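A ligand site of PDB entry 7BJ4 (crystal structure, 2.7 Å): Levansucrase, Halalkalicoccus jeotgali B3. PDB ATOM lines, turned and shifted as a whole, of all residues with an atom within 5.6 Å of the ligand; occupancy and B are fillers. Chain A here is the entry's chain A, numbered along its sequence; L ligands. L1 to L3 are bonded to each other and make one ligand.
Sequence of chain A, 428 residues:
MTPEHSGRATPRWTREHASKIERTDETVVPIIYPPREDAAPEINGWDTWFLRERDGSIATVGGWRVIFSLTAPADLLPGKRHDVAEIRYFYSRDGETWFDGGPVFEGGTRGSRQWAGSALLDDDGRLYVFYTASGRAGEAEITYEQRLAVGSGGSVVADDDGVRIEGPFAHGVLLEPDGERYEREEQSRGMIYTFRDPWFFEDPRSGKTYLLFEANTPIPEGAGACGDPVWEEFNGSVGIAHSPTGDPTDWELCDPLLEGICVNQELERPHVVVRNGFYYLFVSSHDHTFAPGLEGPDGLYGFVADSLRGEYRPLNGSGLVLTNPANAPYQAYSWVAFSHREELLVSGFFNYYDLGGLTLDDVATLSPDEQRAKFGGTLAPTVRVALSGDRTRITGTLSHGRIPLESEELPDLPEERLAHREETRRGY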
ATOM      1  N   TRP A  46      10.597  -7.291  10.683  1.00  0.00           N
ATOM      2  CA  TRP A  46      10.656  -7.873  12.038  1.00  0.00           C
ATOM      3  C   TRP A  46       9.276  -8.466  12.391  1.00  0.00           C
ATOM      4  O   TRP A  46       8.420  -8.507  11.486  1.00  0.00           O
ATOM      5  CB  TRP A  46      11.127  -6.806  13.037  1.00  0.00           C
ATOM      6  CG  TRP A  46      10.203  -5.636  13.250  1.00  0.00           C
ATOM      7  CD1 TRP A  46       9.445  -5.368  14.350  1.00  0.00           C
ATOM      8  CD2 TRP A  46       9.977  -4.542  12.345  1.00  0.00           C
ATOM      9  NE1 TRP A  46       8.741  -4.217  14.190  1.00  0.00           N
ATOM     10  CE2 TRP A  46       9.049  -3.676  12.964  1.00  0.00           C
ATOM     11  CE3 TRP A  46      10.458  -4.216  11.070  1.00  0.00           C
ATOM     12  CZ2 TRP A  46       8.598  -2.510  12.353  1.00  0.00           C
ATOM     13  CZ3 TRP A  46      10.001  -3.064  10.466  1.00  0.00           C
ATOM     14  CH2 TRP A  46       9.081  -2.225  11.109  1.00  0.00           C
ATOM     15  N   ASP A  47       9.105  -8.943  13.625  1.00  0.00           N
ATOM     16  CA  ASP A  47       7.796  -9.371  14.194  1.00  0.00           C
ATOM     17  C   ASP A  47       6.981 -10.107  13.142  1.00  0.00           C
ATOM     18  O   ASP A  47       6.022  -9.496  12.615  1.00  0.00           O
ATOM     19  CB  ASP A  47       7.033  -8.159  14.738  1.00  0.00           C
ATOM     20  CG  ASP A  47       7.451  -7.747  16.137  1.00  0.00           C
ATOM     21  OD1 ASP A  47       8.669  -7.767  16.409  1.00  0.00           O
ATOM     22  OD2 ASP A  47       6.565  -7.425  16.950  1.00  0.00           O
ATOM     23  N   LEU A  70       5.955  -7.195   9.978  1.00  0.00           N
ATOM     24  CA  LEU A  70       6.017  -5.722  10.067  1.00  0.00           C
ATOM     25  C   LEU A  70       7.242  -5.284   9.257  1.00  0.00           C
ATOM     26  O   LEU A  70       8.301  -5.928   9.404  1.00  0.00           O
ATOM     27  CB  LEU A  70       6.142  -5.278  11.526  1.00  0.00           C
ATOM     28  CG  LEU A  70       4.985  -5.669  12.437  1.00  0.00           C
ATOM     29  CD1 LEU A  70       5.145  -4.996  13.779  1.00  0.00           C
ATOM     30  CD2 LEU A  70       3.642  -5.303  11.810  1.00  0.00           C
ATOM     31  N   ARG A  81      11.386   2.792  12.984  1.00  0.00           N
ATOM     32  CA  ARG A  81      10.601   1.888  12.092  1.00  0.00           C
ATOM     33  C   ARG A  81       9.187   1.660  12.650  1.00  0.00           C
ATOM     34  O   ARG A  81       8.250   1.507  11.855  1.00  0.00           O
ATOM     35  CB  ARG A  81      11.353   0.564  11.850  1.00  0.00           C
ATOM     36  CG  ARG A  81      11.416  -0.390  13.033  1.00  0.00           C
ATOM     37  CD  ARG A  81      12.355  -1.574  12.774  1.00  0.00           C
ATOM     38  NE  ARG A  81      12.344  -2.589  13.821  1.00  0.00           N
ATOM     39  CZ  ARG A  81      13.003  -2.499  14.981  1.00  0.00           C
ATOM     40  NH1 ARG A  81      13.748  -1.442  15.263  1.00  0.00           N
ATOM     41  NH2 ARG A  81      12.931  -3.478  15.876  1.00  0.00           N
ATOM     42  N   HIS A  82       9.033   1.694  13.977  1.00  0.00           N
ATOM     43  CA  HIS A  82       7.781   1.380  14.708  1.00  0.00           C
ATOM     44  C   HIS A  82       6.703   2.425  14.431  1.00  0.00           C
ATOM     45  O   HIS A  82       5.526   2.124  14.672  1.00  0.00           O
ATOM     46  CB  HIS A  82       8.020   1.291  16.213  1.00  0.00           C
ATOM     47  CG  HIS A  82       9.190   0.448  16.569  1.00  0.00           C
ATOM     48  ND1 HIS A  82       9.160  -0.927  16.473  1.00  0.00           N
ATOM     49  CD2 HIS A  82      10.451   0.793  16.904  1.00  0.00           C
ATOM     50  CE1 HIS A  82      10.362  -1.398  16.781  1.00  0.00           C
ATOM     51  NE2 HIS A  82      11.167  -0.365  17.062  1.00  0.00           N
ATOM     52  N   TRP A 115       0.789  -2.903  13.931  1.00  0.00           N
ATOM     53  CA  TRP A 115       1.731  -3.735  14.710  1.00  0.00           C
ATOM     54  C   TRP A 115       1.312  -5.206  14.636  1.00  0.00           C
ATOM     55  O   TRP A 115       0.291  -5.501  13.976  1.00  0.00           O
ATOM     56  CB  TRP A 115       1.845  -3.223  16.147  1.00  0.00           C
ATOM     57  CG  TRP A 115       2.554  -1.908  16.252  1.00  0.00           C
ATOM     58  CD1 TRP A 115       3.165  -1.205  15.245  1.00  0.00           C
ATOM     59  CD2 TRP A 115       2.771  -1.144  17.457  1.00  0.00           C
ATOM     60  NE1 TRP A 115       3.723  -0.062  15.740  1.00  0.00           N
ATOM     61  CE2 TRP A 115       3.504   0.013  17.083  1.00  0.00           C
ATOM     62  CE3 TRP A 115       2.420  -1.317  18.795  1.00  0.00           C
ATOM     63  CZ2 TRP A 115       3.880   0.983  18.011  1.00  0.00           C
ATOM     64  CZ3 TRP A 115       2.786  -0.347  19.714  1.00  0.00           C
ATOM     65  CH2 TRP A 115       3.508   0.779  19.321  1.00  0.00           C
ATOM     66  N   ALA A 116       2.071  -6.086  15.271  1.00  0.00           N
ATOM     67  CA  ALA A 116       2.038  -7.546  15.017  1.00  0.00           C
ATOM     68  C   ALA A 116       0.666  -8.100  15.391  1.00  0.00           C
ATOM     69  O   ALA A 116       0.004  -7.493  16.254  1.00  0.00           O
ATOM     70  CB  ALA A 116       3.133  -8.230  15.794  1.00  0.00           C
ATOM     71  N   TYR A 144       0.102   6.578  20.938  1.00  0.00           N
ATOM     72  CA  TYR A 144       0.484   5.176  21.273  1.00  0.00           C
ATOM     73  C   TYR A 144      -0.748   4.404  21.765  1.00  0.00           C
ATOM     74  O   TYR A 144      -0.624   3.535  22.644  1.00  0.00           O
ATOM     75  CB  TYR A 144       1.653   5.180  22.270  1.00  0.00           C
ATOM     76  CG  TYR A 144       2.899   5.779  21.678  1.00  0.00           C
ATOM     77  CD1 TYR A 144       3.592   5.112  20.683  1.00  0.00           C
ATOM     78  CD2 TYR A 144       3.365   7.020  22.071  1.00  0.00           C
ATOM     79  CE1 TYR A 144       4.727   5.660  20.106  1.00  0.00           C
ATOM     80  CE2 TYR A 144       4.497   7.578  21.497  1.00  0.00           C
ATOM     81  CZ  TYR A 144       5.185   6.896  20.509  1.00  0.00           C
ATOM     82  OH  TYR A 144       6.308   7.415  19.946  1.00  0.00           O
ATOM     83  N   ARG A 196      -2.137  -5.230  22.511  1.00  0.00           N
ATOM     84  CA  ARG A 196      -1.677  -5.503  21.139  1.00  0.00           C
ATOM     85  C   ARG A 196      -1.405  -7.001  20.937  1.00  0.00           C
ATOM     86  O   ARG A 196      -1.599  -7.793  21.880  1.00  0.00           O
ATOM     87  CB  ARG A 196      -0.428  -4.660  20.872  1.00  0.00           C
ATOM     88  CG  ARG A 196       0.694  -4.839  21.886  1.00  0.00           C
ATOM     89  CD  ARG A 196       2.030  -4.431  21.299  1.00  0.00           C
ATOM     90  NE  ARG A 196       3.135  -4.519  22.246  1.00  0.00           N
ATOM     91  CZ  ARG A 196       3.501  -3.546  23.082  1.00  0.00           C
ATOM     92  NH1 ARG A 196       2.858  -2.393  23.094  1.00  0.00           N
ATOM     93  NH2 ARG A 196       4.520  -3.722  23.897  1.00  0.00           N
ATOM     94  N   ASP A 197      -0.966  -7.348  19.723  1.00  0.00           N
ATOM     95  CA  ASP A 197      -0.419  -8.680  19.359  1.00  0.00           C
ATOM     96  C   ASP A 197      -1.548  -9.701  19.508  1.00  0.00           C
ATOM     97  O   ASP A 197      -1.432 -10.643  20.296  1.00  0.00           O
ATOM     98  CB  ASP A 197       0.854  -8.966  20.158  1.00  0.00           C
ATOM     99  CG  ASP A 197       1.998  -7.957  19.953  1.00  0.00           C
ATOM    100  OD1 ASP A 197       1.977  -7.244  18.900  1.00  0.00           O
ATOM    101  OD2 ASP A 197       2.914  -7.873  20.813  1.00  0.00           O
ATOM    102  N   GLU A 214      -1.431  -9.337  24.308  1.00  0.00           N
ATOM    103  CA  GLU A 214      -0.645  -8.712  25.375  1.00  0.00           C
ATOM    104  C   GLU A 214      -1.443  -7.523  25.884  1.00  0.00           C
ATOM    105  O   GLU A 214      -1.890  -6.727  25.050  1.00  0.00           O
ATOM    106  CB  GLU A 214       0.724  -8.245  24.884  1.00  0.00           C
ATOM    107  CG  GLU A 214       1.476  -7.476  25.940  1.00  0.00           C
ATOM    108  CD  GLU A 214       2.697  -6.735  25.429  1.00  0.00           C
ATOM    109  OE1 GLU A 214       2.929  -6.756  24.182  1.00  0.00           O
ATOM    110  OE2 GLU A 214       3.404  -6.149  26.283  1.00  0.00           O
ATOM    111  N   GLU A 266       5.974  -5.637  29.798  1.00  0.00           N
ATOM    112  CA  GLU A 266       5.715  -6.125  28.419  1.00  0.00           C
ATOM    113  C   GLU A 266       5.878  -7.649  28.373  1.00  0.00           C
ATOM    114  O   GLU A 266       7.043  -8.125  28.361  1.00  0.00           O
ATOM    115  CB  GLU A 266       6.641  -5.392  27.429  1.00  0.00           C
ATOM    116  CG  GLU A 266       6.216  -3.954  27.149  1.00  0.00           C
ATOM    117  CD  GLU A 266       7.053  -3.171  26.148  1.00  0.00           C
ATOM    118  OE1 GLU A 266       8.156  -3.632  25.791  1.00  0.00           O
ATOM    119  OE2 GLU A 266       6.586  -2.093  25.712  1.00  0.00           O
ATOM    120  N   GLU A 268       5.208  -9.746  25.607  1.00  0.00           N
ATOM    121  CA  GLU A 268       4.931  -9.473  24.175  1.00  0.00           C
ATOM    122  C   GLU A 268       4.599 -10.756  23.398  1.00  0.00           C
ATOM    123  O   GLU A 268       5.017 -11.844  23.814  1.00  0.00           O
ATOM    124  CB  GLU A 268       6.115  -8.775  23.510  1.00  0.00           C
ATOM    125  CG  GLU A 268       6.397  -7.386  24.059  1.00  0.00           C
ATOM    126  CD  GLU A 268       7.006  -6.474  23.005  1.00  0.00           C
ATOM    127  OE1 GLU A 268       6.664  -6.639  21.812  1.00  0.00           O
ATOM    128  OE2 GLU A 268       7.820  -5.609  23.387  1.00  0.00           O
ATOM    129  N   ARG A 269       3.912 -10.591  22.267  1.00  0.00           N
ATOM    130  CA  ARG A 269       3.516 -11.630  21.290  1.00  0.00           C
ATOM    131  C   ARG A 269       3.282 -12.955  22.000  1.00  0.00           C
ATOM    132  O   ARG A 269       4.076 -13.879  21.852  1.00  0.00           O
ATOM    133  CB  ARG A 269       4.573 -11.748  20.187  1.00  0.00           C
ATOM    134  CG  ARG A 269       4.345 -10.704  19.114  1.00  0.00           C
ATOM    135  CD  ARG A 269       5.414 -10.593  18.061  1.00  0.00           C
ATOM    136  NE  ARG A 269       5.586 -11.745  17.191  1.00  0.00           N
ATOM    137  CZ  ARG A 269       4.642 -12.315  16.441  1.00  0.00           C
ATOM    138  NH1 ARG A 269       3.374 -11.915  16.492  1.00  0.00           N
ATOM    139  NH2 ARG A 269       4.973 -13.341  15.686  1.00  0.00           N
ATOM    140  N   HIS A 286      11.614  -7.915  27.181  1.00  0.00           N
ATOM    141  CA  HIS A 286      12.877  -7.128  27.198  1.00  0.00           C
ATOM    142  C   HIS A 286      13.538  -7.156  28.576  1.00  0.00           C
ATOM    143  O   HIS A 286      12.846  -7.464  29.560  1.00  0.00           O
ATOM    144  CB  HIS A 286      12.620  -5.685  26.783  1.00  0.00           C
ATOM    145  CG  HIS A 286      12.198  -5.552  25.375  1.00  0.00           C
ATOM    146  ND1 HIS A 286      10.891  -5.311  25.034  1.00  0.00           N
ATOM    147  CD2 HIS A 286      12.913  -5.611  24.220  1.00  0.00           C
ATOM    148  CE1 HIS A 286      10.811  -5.236  23.711  1.00  0.00           C
ATOM    149  NE2 HIS A 286      12.035  -5.409  23.205  1.00  0.00           N
ATOM    150  N   HIS A 288      14.800  -4.272  29.768  1.00  0.00           N
ATOM    151  CA  HIS A 288      14.487  -2.925  30.296  1.00  0.00           C
ATOM    152  C   HIS A 288      13.052  -2.880  30.824  1.00  0.00           C
ATOM    153  O   HIS A 288      12.739  -1.908  31.522  1.00  0.00           O
ATOM    154  CB  HIS A 288      14.774  -1.820  29.274  1.00  0.00           C
ATOM    155  CG  HIS A 288      13.911  -1.824  28.048  1.00  0.00           C
ATOM    156  ND1 HIS A 288      12.593  -1.365  28.066  1.00  0.00           N
ATOM    157  CD2 HIS A 288      14.202  -2.134  26.771  1.00  0.00           C
ATOM    158  CE1 HIS A 288      12.101  -1.416  26.842  1.00  0.00           C
ATOM    159  NE2 HIS A 288      13.075  -1.880  26.016  1.00  0.00           N
ATOM    160  N   THR A 289      12.224  -3.873  30.534  1.00  0.00           N
ATOM    161  CA  THR A 289      10.797  -3.884  30.964  1.00  0.00           C
ATOM    162  C   THR A 289      10.641  -4.681  32.266  1.00  0.00           C
ATOM    163  O   THR A 289       9.491  -4.874  32.690  1.00  0.00           O
ATOM    164  CB  THR A 289       9.891  -4.426  29.856  1.00  0.00           C
ATOM    165  OG1 THR A 289      10.318  -5.744  29.503  1.00  0.00           O
ATOM    166  CG2 THR A 289       9.904  -3.543  28.628  1.00  0.00           C
ATOM    167  N   ASP A 298      16.642  -9.831  27.454  1.00  0.00           N
ATOM    168  CA  ASP A 298      15.834  -9.978  26.216  1.00  0.00           C
ATOM    169  C   ASP A 298      15.755 -11.490  25.941  1.00  0.00           C
ATOM    170  O   ASP A 298      16.824 -12.123  25.800  1.00  0.00           O
ATOM    171  CB  ASP A 298      16.441  -9.220  25.017  1.00  0.00           C
ATOM    172  CG  ASP A 298      15.971  -7.777  24.783  1.00  0.00           C
ATOM    173  OD1 ASP A 298      15.765  -7.057  25.789  1.00  0.00           O
ATOM    174  OD2 ASP A 298      15.840  -7.373  23.582  1.00  0.00           O
ATOM    175  N   TYR A 330      21.264  -8.538  22.036  1.00  0.00           N
ATOM    176  CA  TYR A 330      20.059  -8.005  21.361  1.00  0.00           C
ATOM    177  C   TYR A 330      19.964  -8.547  19.936  1.00  0.00           C
ATOM    178  O   TYR A 330      19.198  -7.975  19.158  1.00  0.00           O
ATOM    179  CB  TYR A 330      20.084  -6.480  21.384  1.00  0.00           C
ATOM    180  CG  TYR A 330      20.195  -5.886  22.759  1.00  0.00           C
ATOM    181  CD1 TYR A 330      19.197  -6.084  23.701  1.00  0.00           C
ATOM    182  CD2 TYR A 330      21.297  -5.134  23.132  1.00  0.00           C
ATOM    183  CE1 TYR A 330      19.284  -5.543  24.970  1.00  0.00           C
ATOM    184  CE2 TYR A 330      21.393  -4.591  24.402  1.00  0.00           C
ATOM    185  CZ  TYR A 330      20.400  -4.804  25.328  1.00  0.00           C
ATOM    186  OH  TYR A 330      20.497  -4.262  26.566  1.00  0.00           O
ATOM    187  N   TYR A 333      14.927 -11.184  18.621  1.00  0.00           N
ATOM    188  CA  TYR A 333      13.736 -10.861  19.435  1.00  0.00           C
ATOM    189  C   TYR A 333      12.477 -11.328  18.693  1.00  0.00           C
ATOM    190  O   TYR A 333      12.605 -11.789  17.534  1.00  0.00           O
ATOM    191  CB  TYR A 333      13.701  -9.355  19.758  1.00  0.00           C
ATOM    192  CG  TYR A 333      12.680  -8.980  20.802  1.00  0.00           C
ATOM    193  CD1 TYR A 333      12.866  -9.328  22.128  1.00  0.00           C
ATOM    194  CD2 TYR A 333      11.492  -8.352  20.452  1.00  0.00           C
ATOM    195  CE1 TYR A 333      11.917  -9.048  23.089  1.00  0.00           C
ATOM    196  CE2 TYR A 333      10.537  -8.050  21.410  1.00  0.00           C
ATOM    197  CZ  TYR A 333      10.751  -8.389  22.736  1.00  0.00           C
ATOM    198  OH  TYR A 333       9.817  -8.088  23.682  1.00  0.00           O
ATOM    199  N   SER A 334      11.318 -11.235  19.361  1.00  0.00           N
ATOM    200  CA  SER A 334       9.949 -11.459  18.827  1.00  0.00           C
ATOM    201  C   SER A 334       9.848 -12.887  18.275  1.00  0.00           C
ATOM    202  O   SER A 334       9.439 -13.073  17.082  1.00  0.00           O
ATOM    203  CB  SER A 334       9.579 -10.432  17.810  1.00  0.00           C
ATOM    204  OG  SER A 334       8.269 -10.679  17.307  1.00  0.00           O
ATOM    205  N   PHE A 349      13.370 -12.645  14.718  1.00  0.00           N
ATOM    206  CA  PHE A 349      14.026 -11.848  13.661  1.00  0.00           C
ATOM    207  C   PHE A 349      15.399 -11.403  14.150  1.00  0.00           C
ATOM    208  O   PHE A 349      15.638 -11.378  15.375  1.00  0.00           O
ATOM    209  CB  PHE A 349      13.138 -10.668  13.241  1.00  0.00           C
ATOM    210  CG  PHE A 349      13.126  -9.528  14.211  1.00  0.00           C
ATOM    211  CD1 PHE A 349      12.253  -9.532  15.299  1.00  0.00           C
ATOM    212  CD2 PHE A 349      13.975  -8.452  14.055  1.00  0.00           C
ATOM    213  CE1 PHE A 349      12.244  -8.468  16.197  1.00  0.00           C
ATOM    214  CE2 PHE A 349      13.959  -7.398  14.941  1.00  0.00           C
ATOM    215  CZ  PHE A 349      13.088  -7.406  16.006  1.00  0.00           C
ATOM    216  N   ASN A 351      17.854  -8.803  15.067  1.00  0.00           N
ATOM    217  CA  ASN A 351      17.575  -7.467  15.673  1.00  0.00           C
ATOM    218  C   ASN A 351      18.847  -6.604  15.586  1.00  0.00           C
ATOM    219  O   ASN A 351      19.233  -6.250  14.450  1.00  0.00           O
ATOM    220  CB  ASN A 351      17.001  -7.633  17.080  1.00  0.00           C
ATOM    221  CG  ASN A 351      16.419  -6.366  17.668  1.00  0.00           C
ATOM    222  OD1 ASN A 351      15.948  -5.498  16.938  1.00  0.00           O
ATOM    223  ND2 ASN A 351      16.418  -6.281  18.988  1.00  0.00           N
ATOM    224  N   TYR A 352      19.468  -6.256  16.714  1.00  0.00           N
ATOM    225  CA  TYR A 352      20.674  -5.392  16.777  1.00  0.00           C
ATOM    226  C   TYR A 352      21.902  -6.249  17.094  1.00  0.00           C
ATOM    227  O   TYR A 352      21.888  -7.016  18.073  1.00  0.00           O
ATOM    228  CB  TYR A 352      20.524  -4.287  17.831  1.00  0.00           C
ATOM    229  CG  TYR A 352      19.522  -3.212  17.494  1.00  0.00           C
ATOM    230  CD1 TYR A 352      19.863  -2.158  16.673  1.00  0.00           C
ATOM    231  CD2 TYR A 352      18.247  -3.243  18.012  1.00  0.00           C
ATOM    232  CE1 TYR A 352      18.946  -1.154  16.374  1.00  0.00           C
ATOM    233  CE2 TYR A 352      17.324  -2.256  17.729  1.00  0.00           C
ATOM    234  CZ  TYR A 352      17.668  -1.211  16.906  1.00  0.00           C
ATOM    235  OH  TYR A 352      16.746  -0.230  16.642  1.00  0.00           O
ATOM    236  N   LEU A 360      21.363  -0.079  23.786  1.00  0.00           N
ATOM    237  CA  LEU A 360      20.462   0.235  22.657  1.00  0.00           C
ATOM    238  C   LEU A 360      20.189   1.747  22.625  1.00  0.00           C
ATOM    239  O   LEU A 360      20.103   2.303  21.514  1.00  0.00           O
ATOM    240  CB  LEU A 360      19.160  -0.565  22.794  1.00  0.00           C
ATOM    241  CG  LEU A 360      19.253  -2.017  22.347  1.00  0.00           C
ATOM    242  CD1 LEU A 360      17.936  -2.740  22.579  1.00  0.00           C
ATOM    243  CD2 LEU A 360      19.685  -2.133  20.895  1.00  0.00           C
ATOM    244  N   ASP A 361      20.060   2.380  23.789  1.00  0.00           N
ATOM    245  CA  ASP A 361      19.872   3.849  23.884  1.00  0.00           C
ATOM    246  C   ASP A 361      21.060   4.537  23.186  1.00  0.00           C
ATOM    247  O   ASP A 361      20.810   5.436  22.365  1.00  0.00           O
ATOM    248  CB  ASP A 361      19.673   4.291  25.334  1.00  0.00           C
ATOM    249  CG  ASP A 361      18.221   4.191  25.784  1.00  0.00           C
ATOM    250  OD1 ASP A 361      17.501   3.333  25.252  1.00  0.00           O
ATOM    251  OD2 ASP A 361      17.801   4.995  26.641  1.00  0.00           O
HETATM  252  C1  LIG L   1      11.745  -2.111  20.186  1.00  0.00           C
HETATM  253  C2  LIG L   1      12.534  -3.270  19.602  1.00  0.00           C
HETATM  254  C3  LIG L   1      13.557  -3.799  20.591  1.00  0.00           C
HETATM  255  C4  LIG L   1      14.376  -2.659  21.192  1.00  0.00           C
HETATM  256  C5  LIG L   1      13.476  -1.542  21.689  1.00  0.00           C
HETATM  257  C6  LIG L   1      14.297  -0.371  22.225  1.00  0.00           C
HETATM  258  O1  LIG L   1      11.643  -4.324  19.227  1.00  0.00           O
HETATM  259  O2  LIG L   1      14.440  -4.721  19.930  1.00  0.00           O
HETATM  260  O3  LIG L   1      15.159  -3.164  22.288  1.00  0.00           O
HETATM  261  O4  LIG L   1      12.638  -1.096  20.623  1.00  0.00           O
HETATM  262  O5  LIG L   1      13.492   0.426  23.097  1.00  0.00           O
HETATM  263  C1  LG2 L   2       9.171  -3.558  20.042  1.00  0.00           C
HETATM  264  C2  LG2 L   2       9.567  -2.485  21.049  1.00  0.00           C
HETATM  265  C3  LG2 L   2       8.745  -2.625  22.325  1.00  0.00           C
HETATM  266  C4  LG2 L   2       7.866  -1.392  22.406  1.00  0.00           C
HETATM  267  C5  LG2 L   2       8.230  -0.528  21.211  1.00  0.00           C
HETATM  268  C6  LG2 L   2       8.716   0.848  21.649  1.00  0.00           C
HETATM  269  O1  LG2 L   2       7.792  -3.877  20.200  1.00  0.00           O
HETATM  270  O2  LG2 L   2      10.976  -2.579  21.298  1.00  0.00           O
HETATM  271  O3  LG2 L   2       9.554  -2.713  23.510  1.00  0.00           O
HETATM  272  O4  LG2 L   2       6.487  -1.771  22.319  1.00  0.00           O
HETATM  273  O5  LG2 L   2       9.276  -1.196  20.491  1.00  0.00           O
HETATM  274  O6  LG2 L   2       7.620   1.584  22.193  1.00  0.00           O
HETATM  275  C1  LG3 L   3       8.157  -5.971  19.074  1.00  0.00           C
HETATM  276  C2  LG3 L   3       7.309  -4.702  19.141  1.00  0.00           C
HETATM  277  C3  LG3 L   3       5.835  -5.056  19.317  1.00  0.00           C
HETATM  278  C4  LG3 L   3       5.107  -4.422  18.137  1.00  0.00           C
HETATM  279  C5  LG3 L   3       6.173  -3.772  17.282  1.00  0.00           C
HETATM  280  C6  LG3 L   3       5.917  -2.277  17.139  1.00  0.00           C
HETATM  281  O1  LG3 L   3       9.388  -5.690  18.398  1.00  0.00           O
HETATM  282  O2  LG3 L   3       5.281  -4.575  20.543  1.00  0.00           O
HETATM  283  O3  LG3 L   3       4.417  -5.435  17.386  1.00  0.00           O
HETATM  284  O4  LG3 L   3       7.437  -3.987  17.902  1.00  0.00           O
HETATM  285  O5  LG3 L   3       6.390  -1.595  18.306  1.00  0.00           O
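The side-chain amide nitrogen of Asn 351 lies within hydrogen-bond range of an oxygen (O2) of LIG L1, 2.7 Å away.
NE of Arg 196 lies within hydrogen-bond range of O2 of LG3 L3 (2.7 Å).
The side-chain carboxylate (OE1) of Glu 268 sits at hydrogen-bond distance from an oxygen (O2) of LG3 L3, at 2.8 Å.
ND1 of His 286 lies close to O3 of LG2 L2 (3.3 Å).
O3 of LG2 L2 sits at hydrogen-bond distance from OE1 of Glu 266 (2.8 Å).
The side-chain carboxylate (OD2) of Asp 47 sits at hydrogen-bond distance from an oxygen (O3) of LG3 L3 (3.0 Å).
O3 of LG3 L3 sits at hydrogen-bond distance from N of Ala 116.
O5 of LG3 L3 is in hydrogen-bond range of ND1 of His 82 (3.4 Å).
O3 of LG3 L3 sits at hydrogen-bond distance from OD1 of Asp 197 (3.4 Å).
The guanidinium group of Arg 196 lies within salt-bridge range of the side-chain carboxylate of Glu 214 (3.0 Å).
The side-chain carboxylate (OE2) of Glu 268 sits close to a ring nitrogen (ND1) of His 286.
OH of Tyr 333 sits at hydrogen-bond distance from OE2 of Glu 268 (3.2 Å).
A ring nitrogen (ND1) of His 286 sits at hydrogen-bond distance from the side-chain carboxylate of Glu 266 (3.3 Å).
The backbone carbonyl oxygen of His 286 lies within hydrogen-bond range of the side-chain hydroxyl of Thr 289 (3.1 Å).
OG of Ser 334 lies within hydrogen-bond range of OD1 of Asp 47 (3.1 Å).
OD2 of Asp 197 lies within hydrogen-bond range of N of Arg 269, 3.2 Å away.
O of Tyr 333 sits at hydrogen-bond distance from N of Phe 349, at 3.0 Å.
NE1 of Trp 46 touches O4 of LG3 L3, 3.9 Å away.
CD1 of Leu 70 touches O3 of LG3 L3, 3.7 Å away.
Arg 81 touches the ligand.
CE2 of Trp 115 touches C6 of LG3 L3, 3.3 Å away.
NE2 of His 288 touches O5 of LIG L1, at 3.7 Å.
Tyr 333 touches the ligand.
CD1 of Leu 360 touches O3 of LIG L1, 2.8 Å away.
Hydrophobic or aromatic side chains that line the ligand: Leu 70, His 82, Trp 115, Ala 116, His 286, Tyr 333 and Leu 360.
Within 4 Å of the ligand: Trp 46, Asp 47, Leu 70, Arg 81, His 82, Trp 115, Ala 116, Arg 196, Asp 197, Glu 266, Glu 268, His 286, His 288, Tyr 333, Asn 351 and Leu 360.
The nearest printed residue that does not touch the ligand is Tyr 352 (4.4 Å).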
